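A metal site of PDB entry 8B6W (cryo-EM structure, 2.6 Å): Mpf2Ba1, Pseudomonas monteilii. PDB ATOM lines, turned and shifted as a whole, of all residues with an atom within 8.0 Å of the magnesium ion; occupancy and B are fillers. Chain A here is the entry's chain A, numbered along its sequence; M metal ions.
The side-chain carboxylate (OD1) of Asp 336 lies close to the backbone NH (N) of Asn 338 (3.4 Å).
ND2 of Asn 338 lies within hydrogen-bond range of O of Asp 344, 2.6 Å away.
The side-chain amide nitrogen (ND2) of Asn 438 is in hydrogen-bond range of the backbone carbonyl oxygen (O) of Asn 444.
The side-chain carboxylate (OD1) of Asp 436 is in hydrogen-bond range of the backbone NH (N) of Asn 438 (2.7 Å).
The side-chain carboxylate (OD2) of Asp 386 lies close to the backbone NH (N) of Asn 388 (3.1 Å).
The side-chain amide nitrogen (ND2) of Asn 388 is in hydrogen-bond range of the backbone carbonyl oxygen (O) of Asp 394, 2.9 Å away.
The backbone NH (N) of Leu 387 sits at hydrogen-bond distance from the backbone carbonyl oxygen (O) of Val 396.
The backbone carbonyl oxygen (O) of Ile 446 lies within hydrogen-bond range of the backbone NH (N) of Leu 437 (2.8 Å).
Six residues have an atom within 4 Å of the magnesium ion: Leu 337, Asn 338, Leu 387, Asn 388, Leu 437 and Asn 438.
The nearest printed residue that does not touch the magnesium ion is Ala 391 (4.3 Å).
The magnesium ion is bound by OD1 of Asn 338.
OD1 of Asn 438 is bound to the magnesium ion (2.0 Å).
O of Leu 337 binds the magnesium ion (2.1 Å).
OD1 of Asn 388 binds the magnesium ion (2.1 Å).
The magnesium ion is bound by O of Leu 387, 2.4 Å away.
Slightly farther from the magnesium ion lies the backbone carbonyl oxygen (O) of Leu 437 (2.7 Å).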
ATOM      1  N   ASP A 336      15.965 -22.099  -1.297  1.00  0.00           N
ATOM      2  CA  ASP A 336      15.461 -22.510  -2.600  1.00  0.00           C
ATOM      3  C   ASP A 336      14.470 -23.655  -2.439  1.00  0.00           C
ATOM      4  O   ASP A 336      14.564 -24.468  -1.519  1.00  0.00           O
ATOM      5  CB  ASP A 336      16.618 -22.890  -3.525  1.00  0.00           C
ATOM      6  CG  ASP A 336      17.111 -24.318  -3.311  1.00  0.00           C
ATOM      7  OD1 ASP A 336      16.808 -24.928  -2.279  1.00  0.00           O
ATOM      8  OD2 ASP A 336      17.822 -24.824  -4.208  1.00  0.00           O
ATOM      9  N   LEU A 337      13.486 -23.688  -3.328  1.00  0.00           N
ATOM     10  CA  LEU A 337      12.409 -24.653  -3.248  1.00  0.00           C
ATOM     11  C   LEU A 337      12.827 -26.061  -3.699  1.00  0.00           C
ATOM     12  O   LEU A 337      11.950 -26.905  -3.930  1.00  0.00           O
ATOM     13  CB  LEU A 337      11.211 -24.174  -4.071  1.00  0.00           C
ATOM     14  CG  LEU A 337      10.332 -23.160  -3.328  1.00  0.00           C
ATOM     15  CD1 LEU A 337       9.693 -23.765  -2.094  1.00  0.00           C
ATOM     16  CD2 LEU A 337      11.125 -21.908  -2.960  1.00  0.00           C
ATOM     17  N   ASN A 338      14.131 -26.331  -3.827  1.00  0.00           N
ATOM     18  CA  ASN A 338      14.632 -27.675  -4.049  1.00  0.00           C
ATOM     19  C   ASN A 338      15.802 -28.009  -3.129  1.00  0.00           C
ATOM     20  O   ASN A 338      16.587 -28.919  -3.439  1.00  0.00           O
ATOM     21  CB  ASN A 338      15.059 -27.847  -5.519  1.00  0.00           C
ATOM     22  CG  ASN A 338      13.873 -27.889  -6.455  1.00  0.00           C
ATOM     23  OD1 ASN A 338      12.813 -28.424  -6.121  1.00  0.00           O
ATOM     24  ND2 ASN A 338      14.049 -27.322  -7.643  1.00  0.00           N
ATOM     25  N   ALA A 339      15.930 -27.308  -2.005  1.00  0.00           N
ATOM     26  CA  ALA A 339      17.056 -27.528  -1.098  1.00  0.00           C
ATOM     27  C   ALA A 339      17.180 -28.996  -0.722  1.00  0.00           C
ATOM     28  O   ALA A 339      16.223 -29.612  -0.241  1.00  0.00           O
ATOM     29  CB  ALA A 339      16.894 -26.678   0.160  1.00  0.00           C
ATOM     30  N   ALA A 341      17.466 -31.351  -2.868  1.00  0.00           N
ATOM     31  CA  ALA A 341      17.102 -32.114  -4.053  1.00  0.00           C
ATOM     32  C   ALA A 341      18.088 -31.842  -5.184  1.00  0.00           C
ATOM     33  O   ALA A 341      18.929 -30.941  -5.115  1.00  0.00           O
ATOM     34  CB  ALA A 341      15.677 -31.782  -4.486  1.00  0.00           C
ATOM     35  N   GLY A 342      17.974 -32.648  -6.225  1.00  0.00           N
ATOM     36  CA  GLY A 342      18.591 -32.335  -7.498  1.00  0.00           C
ATOM     37  C   GLY A 342      17.845 -31.235  -8.239  1.00  0.00           C
ATOM     38  O   GLY A 342      16.885 -30.634  -7.745  1.00  0.00           O
ATOM     39  N   ASP A 344      17.424 -27.609 -10.551  1.00  0.00           N
ATOM     40  CA  ASP A 344      17.717 -26.186 -10.379  1.00  0.00           C
ATOM     41  C   ASP A 344      17.257 -25.695  -9.013  1.00  0.00           C
ATOM     42  O   ASP A 344      16.224 -26.108  -8.498  1.00  0.00           O
ATOM     43  CB  ASP A 344      17.029 -25.373 -11.477  1.00  0.00           C
ATOM     44  CG  ASP A 344      17.786 -25.428 -12.788  1.00  0.00           C
ATOM     45  OD1 ASP A 344      18.937 -25.893 -12.804  1.00  0.00           O
ATOM     46  OD2 ASP A 344      17.211 -25.004 -13.813  1.00  0.00           O
ATOM     47  N   ILE A 346      15.358 -23.153  -7.231  1.00  0.00           N
ATOM     48  CA  ILE A 346      14.254 -22.243  -7.549  1.00  0.00           C
ATOM     49  C   ILE A 346      13.942 -21.430  -6.309  1.00  0.00           C
ATOM     50  O   ILE A 346      13.825 -21.978  -5.202  1.00  0.00           O
ATOM     51  CB  ILE A 346      13.007 -23.021  -8.009  1.00  0.00           C
ATOM     52  CG1 ILE A 346      13.360 -23.977  -9.156  1.00  0.00           C
ATOM     53  CG2 ILE A 346      11.912 -22.066  -8.438  1.00  0.00           C
ATOM     54  CD1 ILE A 346      13.979 -23.305 -10.366  1.00  0.00           C
ATOM     55  N   ASP A 386       7.861 -24.435 -12.852  1.00  0.00           N
ATOM     56  CA  ASP A 386       7.851 -25.595 -11.971  1.00  0.00           C
ATOM     57  C   ASP A 386       8.953 -25.478 -10.935  1.00  0.00           C
ATOM     58  O   ASP A 386      10.148 -25.510 -11.267  1.00  0.00           O
ATOM     59  CB  ASP A 386       8.002 -26.880 -12.778  1.00  0.00           C
ATOM     60  CG  ASP A 386       8.131 -28.098 -11.890  1.00  0.00           C
ATOM     61  OD1 ASP A 386       7.142 -28.418 -11.182  1.00  0.00           O
ATOM     62  OD2 ASP A 386       9.203 -28.720 -11.876  1.00  0.00           O
ATOM     63  N   LEU A 387       8.562 -25.325  -9.674  1.00  0.00           N
ATOM     64  CA  LEU A 387       9.493 -25.286  -8.552  1.00  0.00           C
ATOM     65  C   LEU A 387      10.014 -26.661  -8.137  1.00  0.00           C
ATOM     66  O   LEU A 387      10.615 -26.790  -7.064  1.00  0.00           O
ATOM     67  CB  LEU A 387       8.817 -24.603  -7.356  1.00  0.00           C
ATOM     68  CG  LEU A 387       7.597 -25.316  -6.784  1.00  0.00           C
ATOM     69  CD1 LEU A 387       7.986 -26.357  -5.733  1.00  0.00           C
ATOM     70  CD2 LEU A 387       6.610 -24.316  -6.215  1.00  0.00           C
ATOM     71  N   ASN A 388       9.803 -27.689  -8.968  1.00  0.00           N
ATOM     72  CA  ASN A 388      10.494 -28.958  -8.832  1.00  0.00           C
ATOM     73  C   ASN A 388      11.312 -29.338 -10.063  1.00  0.00           C
ATOM     74  O   ASN A 388      11.689 -30.502 -10.209  1.00  0.00           O
ATOM     75  CB  ASN A 388       9.485 -30.076  -8.520  1.00  0.00           C
ATOM     76  CG  ASN A 388       8.944 -29.993  -7.116  1.00  0.00           C
ATOM     77  OD1 ASN A 388       9.568 -29.397  -6.231  1.00  0.00           O
ATOM     78  ND2 ASN A 388       7.785 -30.586  -6.889  1.00  0.00           N
ATOM     79  N   LYS A 389      11.599 -28.386 -10.950  1.00  0.00           N
ATOM     80  CA  LYS A 389      12.312 -28.700 -12.183  1.00  0.00           C
ATOM     81  C   LYS A 389      13.655 -29.355 -11.878  1.00  0.00           C
ATOM     82  O   LYS A 389      14.532 -28.734 -11.254  1.00  0.00           O
ATOM     83  CB  LYS A 389      12.514 -27.457 -13.035  1.00  0.00           C
ATOM     84  CG  LYS A 389      12.932 -27.769 -14.458  1.00  0.00           C
ATOM     85  CD  LYS A 389      13.023 -26.525 -15.336  1.00  0.00           C
ATOM     86  CE  LYS A 389      14.164 -25.619 -14.931  1.00  0.00           C
ATOM     87  NZ  LYS A 389      15.486 -26.156 -15.381  1.00  0.00           N
ATOM     88  N   GLY A 390      13.813 -30.602 -12.317  1.00  0.00           N
ATOM     89  CA  GLY A 390      14.958 -31.408 -12.005  1.00  0.00           C
ATOM     90  C   GLY A 390      14.959 -32.014 -10.615  1.00  0.00           C
ATOM     91  O   GLY A 390      15.859 -32.815 -10.309  1.00  0.00           O
ATOM     92  N   ALA A 391      14.005 -31.650  -9.763  1.00  0.00           N
ATOM     93  CA  ALA A 391      13.903 -32.265  -8.446  1.00  0.00           C
ATOM     94  C   ALA A 391      13.179 -33.599  -8.488  1.00  0.00           C
ATOM     95  O   ALA A 391      13.178 -34.328  -7.488  1.00  0.00           O
ATOM     96  CB  ALA A 391      13.180 -31.321  -7.482  1.00  0.00           C
ATOM     97  N   GLY A 392      12.565 -33.940  -9.619  1.00  0.00           N
ATOM     98  CA  GLY A 392      11.652 -35.057  -9.701  1.00  0.00           C
ATOM     99  C   GLY A 392      10.320 -34.757  -9.059  1.00  0.00           C
ATOM    100  O   GLY A 392       9.934 -33.599  -8.826  1.00  0.00           O
ATOM    101  N   ASP A 394       6.148 -34.691  -8.479  1.00  0.00           N
ATOM    102  CA  ASP A 394       5.108 -34.003  -9.236  1.00  0.00           C
ATOM    103  C   ASP A 394       5.584 -32.617  -9.665  1.00  0.00           C
ATOM    104  O   ASP A 394       6.405 -31.980  -9.007  1.00  0.00           O
ATOM    105  CB  ASP A 394       3.839 -33.869  -8.388  1.00  0.00           C
ATOM    106  CG  ASP A 394       3.282 -35.208  -7.967  1.00  0.00           C
ATOM    107  OD1 ASP A 394       3.563 -36.221  -8.655  1.00  0.00           O
ATOM    108  OD2 ASP A 394       2.550 -35.257  -6.949  1.00  0.00           O
ATOM    109  N   VAL A 396       4.921 -28.831  -9.692  1.00  0.00           N
ATOM    110  CA  VAL A 396       4.275 -28.002  -8.684  1.00  0.00           C
ATOM    111  C   VAL A 396       4.437 -26.537  -9.051  1.00  0.00           C
ATOM    112  O   VAL A 396       5.476 -26.117  -9.570  1.00  0.00           O
ATOM    113  CB  VAL A 396       4.846 -28.277  -7.274  1.00  0.00           C
ATOM    114  CG1 VAL A 396       4.080 -27.495  -6.227  1.00  0.00           C
ATOM    115  CG2 VAL A 396       4.804 -29.765  -6.972  1.00  0.00           C
ATOM    116  N   ASP A 436       3.153 -30.086  -0.418  1.00  0.00           N
ATOM    117  CA  ASP A 436       4.603 -30.005  -0.309  1.00  0.00           C
ATOM    118  C   ASP A 436       5.209 -29.440  -1.596  1.00  0.00           C
ATOM    119  O   ASP A 436       4.943 -29.929  -2.693  1.00  0.00           O
ATOM    120  CB  ASP A 436       5.185 -31.394  -0.025  1.00  0.00           C
ATOM    121  CG  ASP A 436       6.689 -31.389   0.127  1.00  0.00           C
ATOM    122  OD1 ASP A 436       7.282 -30.282   0.164  1.00  0.00           O
ATOM    123  OD2 ASP A 436       7.290 -32.475   0.205  1.00  0.00           O
ATOM    124  N   LEU A 437       6.018 -28.396  -1.438  1.00  0.00           N
ATOM    125  CA  LEU A 437       6.794 -27.798  -2.519  1.00  0.00           C
ATOM    126  C   LEU A 437       7.964 -28.670  -2.975  1.00  0.00           C
ATOM    127  O   LEU A 437       8.746 -28.238  -3.823  1.00  0.00           O
ATOM    128  CB  LEU A 437       7.292 -26.418  -2.077  1.00  0.00           C
ATOM    129  CG  LEU A 437       6.141 -25.463  -1.748  1.00  0.00           C
ATOM    130  CD1 LEU A 437       6.633 -24.147  -1.179  1.00  0.00           C
ATOM    131  CD2 LEU A 437       5.298 -25.211  -2.980  1.00  0.00           C
ATOM    132  N   ASN A 438       8.087 -29.873  -2.414  1.00  0.00           N
ATOM    133  CA  ASN A 438       8.879 -30.948  -3.002  1.00  0.00           C
ATOM    134  C   ASN A 438       8.061 -32.227  -3.072  1.00  0.00           C
ATOM    135  O   ASN A 438       8.587 -33.331  -2.928  1.00  0.00           O
ATOM    136  CB  ASN A 438      10.171 -31.185  -2.208  1.00  0.00           C
ATOM    137  CG  ASN A 438      11.257 -30.174  -2.549  1.00  0.00           C
ATOM    138  OD1 ASN A 438      11.243 -29.572  -3.619  1.00  0.00           O
ATOM    139  ND2 ASN A 438      12.197 -29.991  -1.638  1.00  0.00           N
ATOM    140  N   ARG A 439       6.755 -32.077  -3.289  1.00  0.00           N
ATOM    141  CA  ARG A 439       5.837 -33.199  -3.426  1.00  0.00           C
ATOM    142  C   ARG A 439       6.423 -34.245  -4.349  1.00  0.00           C
ATOM    143  O   ARG A 439       6.657 -33.997  -5.538  1.00  0.00           O
ATOM    144  CB  ARG A 439       4.502 -32.686  -3.970  1.00  0.00           C
ATOM    145  CG  ARG A 439       3.591 -33.741  -4.595  1.00  0.00           C
ATOM    146  CD  ARG A 439       3.166 -34.779  -3.578  1.00  0.00           C
ATOM    147  NE  ARG A 439       1.946 -34.371  -2.885  1.00  0.00           N
ATOM    148  CZ  ARG A 439       0.732 -34.397  -3.418  1.00  0.00           C
ATOM    149  NH1 ARG A 439       0.524 -34.839  -4.639  1.00  0.00           N
ATOM    150  NH2 ARG A 439      -0.298 -33.972  -2.698  1.00  0.00           N
ATOM    151  N   ALA A 441       9.267 -35.101  -4.742  1.00  0.00           N
ATOM    152  CA  ALA A 441      10.633 -34.816  -5.141  1.00  0.00           C
ATOM    153  C   ALA A 441      11.601 -35.240  -4.058  1.00  0.00           C
ATOM    154  O   ALA A 441      11.219 -35.647  -2.954  1.00  0.00           O
ATOM    155  CB  ALA A 441      10.790 -33.327  -5.454  1.00  0.00           C
ATOM    156  N   GLY A 442      12.892 -35.159  -4.368  1.00  0.00           N
ATOM    157  CA  GLY A 442      13.935 -35.391  -3.393  1.00  0.00           C
ATOM    158  C   GLY A 442      14.003 -34.304  -2.334  1.00  0.00           C
ATOM    159  O   GLY A 442      13.244 -33.338  -2.296  1.00  0.00           O
ATOM    160  N   ASN A 444      14.393 -32.110   1.274  1.00  0.00           N
ATOM    161  CA  ASN A 444      13.502 -31.724   2.354  1.00  0.00           C
ATOM    162  C   ASN A 444      12.068 -31.547   1.857  1.00  0.00           C
ATOM    163  O   ASN A 444      11.816 -31.228   0.692  1.00  0.00           O
ATOM    164  CB  ASN A 444      13.981 -30.412   2.989  1.00  0.00           C
ATOM    165  CG  ASN A 444      15.314 -30.570   3.692  1.00  0.00           C
ATOM    166  OD1 ASN A 444      15.382 -31.116   4.799  1.00  0.00           O
ATOM    167  ND2 ASN A 444      16.382 -30.092   3.059  1.00  0.00           N
ATOM    168  N   ILE A 446       9.172 -28.916   1.966  1.00  0.00           N
ATOM    169  CA  ILE A 446       9.207 -27.456   1.977  1.00  0.00           C
ATOM    170  C   ILE A 446       7.794 -26.934   1.817  1.00  0.00           C
ATOM    171  O   ILE A 446       7.007 -27.468   1.017  1.00  0.00           O
ATOM    172  CB  ILE A 446      10.139 -26.901   0.879  1.00  0.00           C
ATOM    173  CG1 ILE A 446      11.552 -27.473   1.043  1.00  0.00           C
ATOM    174  CG2 ILE A 446      10.159 -25.375   0.936  1.00  0.00           C
ATOM    175  CD1 ILE A 446      12.527 -27.036  -0.029  1.00  0.00           C
HETATM  176 MG    MG M   1      11.094 -28.327  -5.234  1.00  0.00          MG
